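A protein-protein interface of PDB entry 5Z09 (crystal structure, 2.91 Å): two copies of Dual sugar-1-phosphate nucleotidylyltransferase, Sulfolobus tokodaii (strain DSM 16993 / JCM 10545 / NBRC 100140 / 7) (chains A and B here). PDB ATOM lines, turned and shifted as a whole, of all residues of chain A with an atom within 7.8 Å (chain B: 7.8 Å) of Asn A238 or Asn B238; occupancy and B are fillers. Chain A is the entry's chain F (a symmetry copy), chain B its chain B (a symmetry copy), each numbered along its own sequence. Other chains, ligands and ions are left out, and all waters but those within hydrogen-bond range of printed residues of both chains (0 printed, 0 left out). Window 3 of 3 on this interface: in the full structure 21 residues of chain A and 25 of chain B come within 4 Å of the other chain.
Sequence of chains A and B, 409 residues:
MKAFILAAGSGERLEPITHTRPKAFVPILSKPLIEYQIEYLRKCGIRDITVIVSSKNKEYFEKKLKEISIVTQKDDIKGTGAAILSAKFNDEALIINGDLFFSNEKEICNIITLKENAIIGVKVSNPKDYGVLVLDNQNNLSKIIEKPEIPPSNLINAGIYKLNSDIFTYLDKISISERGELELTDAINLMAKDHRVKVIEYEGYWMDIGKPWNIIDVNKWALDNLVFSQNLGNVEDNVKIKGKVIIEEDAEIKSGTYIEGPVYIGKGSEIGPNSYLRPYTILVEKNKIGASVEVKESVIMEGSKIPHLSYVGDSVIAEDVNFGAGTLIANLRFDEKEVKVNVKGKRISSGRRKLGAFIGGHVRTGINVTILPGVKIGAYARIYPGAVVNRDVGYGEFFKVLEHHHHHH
The side-chain carboxylate (OE1) of Glu A236 lies within hydrogen-bond range of the side-chain hydroxyl (OH) of Tyr B258, 2.6 Å away.
The side-chain amino group (NZ) of Lys B240 is in hydrogen-bond range of the side-chain hydroxyl (OG) of Ser A255, at 3.0 Å.
The side-chain amide nitrogen of Asn A238 lies close to the side-chain amide nitrogen of Asn B238, 3.5 Å away.
The side-chain amino group (NZ) of Lys B240 is in salt-bridge range of the side-chain carboxylate (OD1) of Asp A237, at 2.9 Å.
The side-chain amide nitrogen of Asn A274 lies within hydrogen-bond range of the backbone carbonyl oxygen of Gly B256 (3.2 Å).
The side-chain amino group (NZ) of Lys B240 lies within salt-bridge range of the side-chain carboxylate (OE1) of Glu A236 (3.5 Å).
The backbone carbonyl oxygen of Asp A237 lies within hydrogen-bond range of the side-chain hydroxyl of Ser A255.
The backbone NH of Glu A236 is in hydrogen-bond range of the backbone carbonyl oxygen of Ile A253.
The side-chain carboxylate of Glu A236 sits at hydrogen-bond distance from the backbone NH of Ser A255.
O of Ser A255 is in hydrogen-bond range of N of Asn A274 (3.1 Å).
N of Lys B240 is in hydrogen-bond range of O of Thr B257.
The backbone NH (N) of Asn B274 sits at hydrogen-bond distance from the backbone carbonyl oxygen (O) of Ser B255 (3.1 Å).
Lys A254 touches Tyr B258 (CB to OH, 3.5 Å).
Ser A255 touches Tyr B258.
OD1 of Asn B274 touches OD1 of Asn A274 (3.6 Å).
Asn A238 touches just one residue of chain B: Asn B238 (3.5 Å).
Of the printed residues of chain A, Asn B238 touches Asn A238 (3.5 Å).
Of the printed residues of chain B, Lys A254 touches Tyr B258.
Of the printed residues of chain B, Ser A255 touches Lys B240 and Tyr B258.
Of the printed residues of chain A, Lys B240 touches Glu A236 (3.5 Å), Asp A237 (2.9 Å) and Ser A255 (3.0 Å).
Along chain A the printed residues that touch a printed residue of chain B span positions 236 to 274.
Of the 14 printed residues of chain B, 5 touch a printed residue of chain A.
Along chain B the printed residues that touch a printed residue of chain A span positions 238 to 274.
Among the printed residues, Asp or Glu carboxylates within 4 Å of a Lys or Arg side-chain nitrogen of the other chain: Glu A236 with Lys B240 (3.5 Å) and Asp A237 with Lys B240 (2.9 Å).
Glu A236 touches Lys B240, but with the chains exchanged Lys A240 does not touch Glu B236 (16.8 Å).
Glu A236 touches Tyr B258, but with the chains exchanged Tyr A258 does not touch Glu B236 (17.3 Å).
Asp A237 touches Lys B240, but with the chains exchanged Lys A240 does not touch Asp B237 (13.9 Å).
Ser A255 touches Lys B240, but with the chains exchanged Lys A240 does not touch Ser B255 (13.8 Å).
14 positions are printed for both chains.
Of the 9 pairs that touch across the chains among the printed residues, 2 have their exchanged pair printed and touching as well.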
ATOM      1  N   VAL A 235     -15.740 -19.141 -13.347  1.00  0.00           N
ATOM      2  CA  VAL A 235     -15.743 -18.430 -12.073  1.00  0.00           C
ATOM      3  C   VAL A 235     -15.562 -16.958 -12.370  1.00  0.00           C
ATOM      4  O   VAL A 235     -14.594 -16.564 -13.004  1.00  0.00           O
ATOM      5  CB  VAL A 235     -14.604 -18.890 -11.133  1.00  0.00           C
ATOM      6  CG1 VAL A 235     -14.596 -18.073  -9.849  1.00  0.00           C
ATOM      7  CG2 VAL A 235     -14.725 -20.374 -10.806  1.00  0.00           C
ATOM      8  N   GLU A 236     -16.468 -16.138 -11.858  1.00  0.00           N
ATOM      9  CA  GLU A 236     -16.377 -14.696 -12.045  1.00  0.00           C
ATOM     10  C   GLU A 236     -15.344 -14.079 -11.095  1.00  0.00           C
ATOM     11  O   GLU A 236     -14.739 -14.763 -10.266  1.00  0.00           O
ATOM     12  CB  GLU A 236     -17.757 -14.048 -11.830  1.00  0.00           C
ATOM     13  CG  GLU A 236     -18.878 -14.717 -12.612  1.00  0.00           C
ATOM     14  CD  GLU A 236     -20.165 -13.898 -12.679  1.00  0.00           C
ATOM     15  OE1 GLU A 236     -20.455 -13.110 -11.759  1.00  0.00           O
ATOM     16  OE2 GLU A 236     -20.938 -14.116 -13.632  1.00  0.00           O
ATOM     17  N   ASP A 237     -15.162 -12.770 -11.211  1.00  0.00           N
ATOM     18  CA  ASP A 237     -14.313 -12.030 -10.292  1.00  0.00           C
ATOM     19  C   ASP A 237     -14.962 -11.922  -8.905  1.00  0.00           C
ATOM     20  O   ASP A 237     -16.143 -12.209  -8.734  1.00  0.00           O
ATOM     21  CB  ASP A 237     -13.993 -10.636 -10.858  1.00  0.00           C
ATOM     22  CG  ASP A 237     -15.135 -10.052 -11.689  1.00  0.00           C
ATOM     23  OD1 ASP A 237     -15.612 -10.747 -12.610  1.00  0.00           O
ATOM     24  OD2 ASP A 237     -15.549  -8.897 -11.434  1.00  0.00           O
ATOM     25  N   ASN A 238     -14.182 -11.464  -7.931  1.00  0.00           N
ATOM     26  CA  ASN A 238     -14.577 -11.479  -6.528  1.00  0.00           C
ATOM     27  C   ASN A 238     -15.251 -12.774  -6.149  1.00  0.00           C
ATOM     28  O   ASN A 238     -16.267 -12.773  -5.451  1.00  0.00           O
ATOM     29  CB  ASN A 238     -15.498 -10.313  -6.199  1.00  0.00           C
ATOM     30  CG  ASN A 238     -15.099  -9.047  -6.916  1.00  0.00           C
ATOM     31  OD1 ASN A 238     -15.939  -8.364  -7.504  1.00  0.00           O
ATOM     32  ND2 ASN A 238     -13.821  -8.689  -6.821  1.00  0.00           N
ATOM     33  N   VAL A 239     -14.615 -13.884  -6.507  1.00  0.00           N
ATOM     34  CA  VAL A 239     -14.919 -15.178  -5.886  1.00  0.00           C
ATOM     35  C   VAL A 239     -13.708 -15.702  -5.143  1.00  0.00           C
ATOM     36  O   VAL A 239     -12.644 -15.790  -5.712  1.00  0.00           O
ATOM     37  CB  VAL A 239     -15.289 -16.211  -6.956  1.00  0.00           C
ATOM     38  CG1 VAL A 239     -15.557 -17.562  -6.315  1.00  0.00           C
ATOM     39  CG2 VAL A 239     -16.493 -15.729  -7.765  1.00  0.00           C
ATOM     40  N   LYS A 240     -13.840 -15.896  -3.843  1.00  0.00           N
ATOM     41  CA  LYS A 240     -12.739 -16.377  -3.027  1.00  0.00           C
ATOM     42  C   LYS A 240     -12.796 -17.901  -2.963  1.00  0.00           C
ATOM     43  O   LYS A 240     -13.852 -18.483  -2.709  1.00  0.00           O
ATOM     44  CB  LYS A 240     -12.812 -15.777  -1.615  1.00  0.00           C
ATOM     45  CG  LYS A 240     -11.613 -16.088  -0.726  1.00  0.00           C
ATOM     46  CD  LYS A 240     -10.314 -15.627  -1.369  1.00  0.00           C
ATOM     47  CE  LYS A 240      -9.301 -15.193  -0.327  1.00  0.00           C
ATOM     48  NZ  LYS A 240      -9.542 -13.785   0.096  1.00  0.00           N
ATOM     49  N   ILE A 241     -11.665 -18.550  -3.209  1.00  0.00           N
ATOM     50  CA  ILE A 241     -11.599 -20.011  -3.157  1.00  0.00           C
ATOM     51  C   ILE A 241     -10.422 -20.491  -2.323  1.00  0.00           C
ATOM     52  O   ILE A 241      -9.301 -20.040  -2.519  1.00  0.00           O
ATOM     53  CB  ILE A 241     -11.474 -20.584  -4.575  1.00  0.00           C
ATOM     54  CG1 ILE A 241     -12.657 -20.103  -5.425  1.00  0.00           C
ATOM     55  CG2 ILE A 241     -11.408 -22.101  -4.519  1.00  0.00           C
ATOM     56  CD1 ILE A 241     -12.931 -20.937  -6.651  1.00  0.00           C
ATOM     57  N   ILE A 253     -20.054 -19.883 -11.265  1.00  0.00           N
ATOM     58  CA  ILE A 253     -19.900 -19.398  -9.912  1.00  0.00           C
ATOM     59  C   ILE A 253     -19.748 -17.884  -9.942  1.00  0.00           C
ATOM     60  O   ILE A 253     -18.744 -17.364 -10.410  1.00  0.00           O
ATOM     61  CB  ILE A 253     -18.679 -20.023  -9.238  1.00  0.00           C
ATOM     62  CG1 ILE A 253     -18.844 -21.542  -9.199  1.00  0.00           C
ATOM     63  CG2 ILE A 253     -18.496 -19.449  -7.844  1.00  0.00           C
ATOM     64  CD1 ILE A 253     -17.640 -22.276  -8.647  1.00  0.00           C
ATOM     65  N   LYS A 254     -20.729 -17.189  -9.377  1.00  0.00           N
ATOM     66  CA  LYS A 254     -20.836 -15.749  -9.542  1.00  0.00           C
ATOM     67  C   LYS A 254     -20.172 -14.962  -8.401  1.00  0.00           C
ATOM     68  O   LYS A 254     -20.022 -15.452  -7.274  1.00  0.00           O
ATOM     69  CB  LYS A 254     -22.302 -15.353  -9.625  1.00  0.00           C
ATOM     70  CG  LYS A 254     -23.048 -15.977 -10.778  1.00  0.00           C
ATOM     71  CD  LYS A 254     -24.523 -15.618 -10.714  1.00  0.00           C
ATOM     72  CE  LYS A 254     -25.313 -16.373 -11.764  1.00  0.00           C
ATOM     73  NZ  LYS A 254     -26.648 -15.769 -11.966  1.00  0.00           N
ATOM     74  N   SER A 255     -19.910 -13.695  -8.684  1.00  0.00           N
ATOM     75  CA  SER A 255     -19.163 -12.831  -7.798  1.00  0.00           C
ATOM     76  C   SER A 255     -19.766 -12.791  -6.400  1.00  0.00           C
ATOM     77  O   SER A 255     -20.989 -12.863  -6.231  1.00  0.00           O
ATOM     78  CB  SER A 255     -19.114 -11.420  -8.388  1.00  0.00           C
ATOM     79  OG  SER A 255     -18.643 -11.450  -9.729  1.00  0.00           O
ATOM     80  N   GLY A 256     -18.896 -12.646  -5.401  1.00  0.00           N
ATOM     81  CA  GLY A 256     -19.323 -12.555  -4.016  1.00  0.00           C
ATOM     82  C   GLY A 256     -19.338 -13.892  -3.301  1.00  0.00           C
ATOM     83  O   GLY A 256     -19.356 -13.965  -2.070  1.00  0.00           O
ATOM     84  N   THR A 257     -19.344 -14.954  -4.081  1.00  0.00           N
ATOM     85  CA  THR A 257     -19.278 -16.288  -3.528  1.00  0.00           C
ATOM     86  C   THR A 257     -17.942 -16.506  -2.808  1.00  0.00           C
ATOM     87  O   THR A 257     -16.907 -15.992  -3.221  1.00  0.00           O
ATOM     88  CB  THR A 257     -19.460 -17.331  -4.638  1.00  0.00           C
ATOM     89  OG1 THR A 257     -20.731 -17.118  -5.258  1.00  0.00           O
ATOM     90  CG2 THR A 257     -19.398 -18.742  -4.081  1.00  0.00           C
ATOM     91  N   TYR A 258     -17.991 -17.322  -1.768  1.00  0.00           N
ATOM     92  CA  TYR A 258     -16.863 -17.553  -0.920  1.00  0.00           C
ATOM     93  C   TYR A 258     -16.873 -19.039  -0.605  1.00  0.00           C
ATOM     94  O   TYR A 258     -17.863 -19.562  -0.085  1.00  0.00           O
ATOM     95  CB  TYR A 258     -17.006 -16.733   0.369  1.00  0.00           C
ATOM     96  CG  TYR A 258     -15.732 -16.608   1.184  1.00  0.00           C
ATOM     97  CD1 TYR A 258     -14.937 -15.472   1.094  1.00  0.00           C
ATOM     98  CD2 TYR A 258     -15.397 -17.563   2.139  1.00  0.00           C
ATOM     99  CE1 TYR A 258     -13.849 -15.294   1.927  1.00  0.00           C
ATOM    100  CE2 TYR A 258     -14.285 -17.412   2.953  1.00  0.00           C
ATOM    101  CZ  TYR A 258     -13.513 -16.279   2.845  1.00  0.00           C
ATOM    102  OH  TYR A 258     -12.386 -16.128   3.625  1.00  0.00           O
ATOM    103  N   ASN A 274     -23.013 -14.049  -4.144  1.00  0.00           N
ATOM    104  CA  ASN A 274     -22.924 -13.985  -2.689  1.00  0.00           C
ATOM    105  C   ASN A 274     -23.438 -15.248  -1.990  1.00  0.00           C
ATOM    106  O   ASN A 274     -24.195 -15.178  -1.029  1.00  0.00           O
ATOM    107  CB  ASN A 274     -23.652 -12.737  -2.202  1.00  0.00           C
ATOM    108  CG  ASN A 274     -22.988 -11.461  -2.699  1.00  0.00           C
ATOM    109  OD1 ASN A 274     -21.830 -11.185  -2.383  1.00  0.00           O
ATOM    110  ND2 ASN A 274     -23.720 -10.670  -3.466  1.00  0.00           N
ATOM    111  N   VAL B 235     -21.399   4.449  -8.112  1.00  0.00           N
ATOM    112  CA  VAL B 235     -21.214   3.018  -7.873  1.00  0.00           C
ATOM    113  C   VAL B 235     -19.838   2.745  -7.264  1.00  0.00           C
ATOM    114  O   VAL B 235     -18.829   3.162  -7.803  1.00  0.00           O
ATOM    115  CB  VAL B 235     -21.316   2.236  -9.192  1.00  0.00           C
ATOM    116  CG1 VAL B 235     -21.093   0.757  -8.949  1.00  0.00           C
ATOM    117  CG2 VAL B 235     -22.669   2.475  -9.856  1.00  0.00           C
ATOM    118  N   GLU B 236     -19.806   2.021  -6.152  1.00  0.00           N
ATOM    119  CA  GLU B 236     -18.550   1.672  -5.474  1.00  0.00           C
ATOM    120  C   GLU B 236     -17.874   0.504  -6.164  1.00  0.00           C
ATOM    121  O   GLU B 236     -18.381  -0.028  -7.153  1.00  0.00           O
ATOM    122  CB  GLU B 236     -18.802   1.330  -3.988  1.00  0.00           C
ATOM    123  CG  GLU B 236     -19.635   2.376  -3.251  1.00  0.00           C
ATOM    124  CD  GLU B 236     -19.630   2.227  -1.735  1.00  0.00           C
ATOM    125  OE1 GLU B 236     -19.440   1.107  -1.224  1.00  0.00           O
ATOM    126  OE2 GLU B 236     -19.853   3.244  -1.051  1.00  0.00           O
ATOM    127  N   ASP B 237     -16.695   0.139  -5.671  1.00  0.00           N
ATOM    128  CA  ASP B 237     -15.970  -1.028  -6.184  1.00  0.00           C
ATOM    129  C   ASP B 237     -16.667  -2.318  -5.750  1.00  0.00           C
ATOM    130  O   ASP B 237     -17.547  -2.301  -4.899  1.00  0.00           O
ATOM    131  CB  ASP B 237     -14.514  -1.018  -5.706  1.00  0.00           C
ATOM    132  CG  ASP B 237     -14.351  -0.392  -4.312  1.00  0.00           C
ATOM    133  OD1 ASP B 237     -14.838   0.744  -4.104  1.00  0.00           O
ATOM    134  OD2 ASP B 237     -13.721  -1.021  -3.430  1.00  0.00           O
ATOM    135  N   ASN B 238     -16.246  -3.429  -6.333  1.00  0.00           N
ATOM    136  CA  ASN B 238     -16.930  -4.709  -6.189  1.00  0.00           C
ATOM    137  C   ASN B 238     -18.432  -4.560  -6.301  1.00  0.00           C
ATOM    138  O   ASN B 238     -19.180  -5.131  -5.508  1.00  0.00           O
ATOM    139  CB  ASN B 238     -16.583  -5.399  -4.867  1.00  0.00           C
ATOM    140  CG  ASN B 238     -15.123  -5.240  -4.489  1.00  0.00           C
ATOM    141  OD1 ASN B 238     -14.806  -4.853  -3.365  1.00  0.00           O
ATOM    142  ND2 ASN B 238     -14.230  -5.516  -5.429  1.00  0.00           N
ATOM    143  N   VAL B 239     -18.876  -3.852  -7.326  1.00  0.00           N
ATOM    144  CA  VAL B 239     -20.261  -3.944  -7.761  1.00  0.00           C
ATOM    145  C   VAL B 239     -20.290  -4.562  -9.141  1.00  0.00           C
ATOM    146  O   VAL B 239     -19.678  -4.037 -10.048  1.00  0.00           O
ATOM    147  CB  VAL B 239     -20.916  -2.551  -7.815  1.00  0.00           C
ATOM    148  CG1 VAL B 239     -22.347  -2.651  -8.320  1.00  0.00           C
ATOM    149  CG2 VAL B 239     -20.865  -1.903  -6.445  1.00  0.00           C
ATOM    150  N   LYS B 240     -20.986  -5.687  -9.285  1.00  0.00           N
ATOM    151  CA  LYS B 240     -21.135  -6.329 -10.584  1.00  0.00           C
ATOM    152  C   LYS B 240     -22.393  -5.820 -11.278  1.00  0.00           C
ATOM    153  O   LYS B 240     -23.466  -5.806 -10.703  1.00  0.00           O
ATOM    154  CB  LYS B 240     -21.174  -7.852 -10.417  1.00  0.00           C
ATOM    155  CG  LYS B 240     -21.096  -8.635 -11.713  1.00  0.00           C
ATOM    156  CD  LYS B 240     -19.860  -8.271 -12.513  1.00  0.00           C
ATOM    157  CE  LYS B 240     -19.348  -9.456 -13.310  1.00  0.00           C
ATOM    158  NZ  LYS B 240     -18.486 -10.331 -12.472  1.00  0.00           N
ATOM    159  N   ILE B 241     -22.257  -5.425 -12.530  1.00  0.00           N
ATOM    160  CA  ILE B 241     -23.400  -4.983 -13.312  1.00  0.00           C
ATOM    161  C   ILE B 241     -23.457  -5.693 -14.669  1.00  0.00           C
ATOM    162  O   ILE B 241     -22.487  -5.700 -15.413  1.00  0.00           O
ATOM    163  CB  ILE B 241     -23.323  -3.466 -13.525  1.00  0.00           C
ATOM    164  CG1 ILE B 241     -23.239  -2.780 -12.163  1.00  0.00           C
ATOM    165  CG2 ILE B 241     -24.516  -2.978 -14.331  1.00  0.00           C
ATOM    166  CD1 ILE B 241     -23.626  -1.321 -12.187  1.00  0.00           C
ATOM    167  N   ILE B 253     -24.787   3.076  -4.934  1.00  0.00           N
ATOM    168  CA  ILE B 253     -24.775   1.618  -5.001  1.00  0.00           C
ATOM    169  C   ILE B 253     -23.497   1.066  -4.407  1.00  0.00           C
ATOM    170  O   ILE B 253     -22.426   1.283  -4.948  1.00  0.00           O
ATOM    171  CB  ILE B 253     -24.893   1.131  -6.458  1.00  0.00           C
ATOM    172  CG1 ILE B 253     -26.200   1.647  -7.066  1.00  0.00           C
ATOM    173  CG2 ILE B 253     -24.818  -0.395  -6.515  1.00  0.00           C
ATOM    174  CD1 ILE B 253     -26.378   1.310  -8.526  1.00  0.00           C
ATOM    175  N   LYS B 254     -23.619   0.298  -3.335  1.00  0.00           N
ATOM    176  CA  LYS B 254     -22.469  -0.011  -2.496  1.00  0.00           C
ATOM    177  C   LYS B 254     -21.887  -1.367  -2.842  1.00  0.00           C
ATOM    178  O   LYS B 254     -22.583  -2.248  -3.326  1.00  0.00           O
ATOM    179  CB  LYS B 254     -22.847   0.024  -1.006  1.00  0.00           C
ATOM    180  CG  LYS B 254     -23.332   1.376  -0.503  1.00  0.00           C
ATOM    181  CD  LYS B 254     -23.803   1.275   0.937  1.00  0.00           C
ATOM    182  CE  LYS B 254     -24.460   2.562   1.389  1.00  0.00           C
ATOM    183  NZ  LYS B 254     -24.587   2.602   2.868  1.00  0.00           N
ATOM    184  N   SER B 255     -20.642  -1.558  -2.427  1.00  0.00           N
ATOM    185  CA  SER B 255     -19.887  -2.755  -2.730  1.00  0.00           C
ATOM    186  C   SER B 255     -20.642  -4.029  -2.372  1.00  0.00           C
ATOM    187  O   SER B 255     -21.347  -4.097  -1.366  1.00  0.00           O
ATOM    188  CB  SER B 255     -18.537  -2.722  -2.000  1.00  0.00           C
ATOM    189  OG  SER B 255     -17.886  -1.487  -2.230  1.00  0.00           O
ATOM    190  N   GLY B 256     -20.461  -5.047  -3.202  1.00  0.00           N
ATOM    191  CA  GLY B 256     -21.021  -6.364  -2.941  1.00  0.00           C
ATOM    192  C   GLY B 256     -22.316  -6.556  -3.691  1.00  0.00           C
ATOM    193  O   GLY B 256     -22.786  -7.685  -3.872  1.00  0.00           O
ATOM    194  N   THR B 257     -22.915  -5.443  -4.092  1.00  0.00           N
ATOM    195  CA  THR B 257     -24.131  -5.477  -4.857  1.00  0.00           C
ATOM    196  C   THR B 257     -23.903  -6.132  -6.203  1.00  0.00           C
ATOM    197  O   THR B 257     -22.836  -6.003  -6.804  1.00  0.00           O
ATOM    198  CB  THR B 257     -24.668  -4.067  -5.067  1.00  0.00           C
ATOM    199  OG1 THR B 257     -24.926  -3.493  -3.783  1.00  0.00           O
ATOM    200  CG2 THR B 257     -25.959  -4.097  -5.876  1.00  0.00           C
ATOM    201  N   TYR B 258     -24.898  -6.900  -6.629  1.00  0.00           N
ATOM    202  CA  TYR B 258     -24.826  -7.679  -7.855  1.00  0.00           C
ATOM    203  C   TYR B 258     -26.122  -7.441  -8.627  1.00  0.00           C
ATOM    204  O   TYR B 258     -27.201  -7.651  -8.093  1.00  0.00           O
ATOM    205  CB  TYR B 258     -24.680  -9.161  -7.493  1.00  0.00           C
ATOM    206  CG  TYR B 258     -24.223 -10.050  -8.607  1.00  0.00           C
ATOM    207  CD1 TYR B 258     -22.892 -10.439  -8.706  1.00  0.00           C
ATOM    208  CD2 TYR B 258     -25.133 -10.557  -9.544  1.00  0.00           C
ATOM    209  CE1 TYR B 258     -22.469 -11.289  -9.718  1.00  0.00           C
ATOM    210  CE2 TYR B 258     -24.720 -11.411 -10.554  1.00  0.00           C
ATOM    211  CZ  TYR B 258     -23.391 -11.777 -10.635  1.00  0.00           C
ATOM    212  OH  TYR B 258     -22.971 -12.613 -11.629  1.00  0.00           O
ATOM    213  N   ASN B 274     -23.944  -5.499  -0.424  1.00  0.00           N
ATOM    214  CA  ASN B 274     -24.375  -6.873  -0.681  1.00  0.00           C
ATOM    215  C   ASN B 274     -25.892  -7.019  -0.927  1.00  0.00           C
ATOM    216  O   ASN B 274     -26.520  -7.934  -0.408  1.00  0.00           O
ATOM    217  CB  ASN B 274     -23.907  -7.755   0.466  1.00  0.00           C
ATOM    218  CG  ASN B 274     -22.392  -7.796   0.580  1.00  0.00           C
ATOM    219  OD1 ASN B 274     -21.697  -8.244  -0.338  1.00  0.00           O
ATOM    220  ND2 ASN B 274     -21.867  -7.313   1.701  1.00  0.00           N
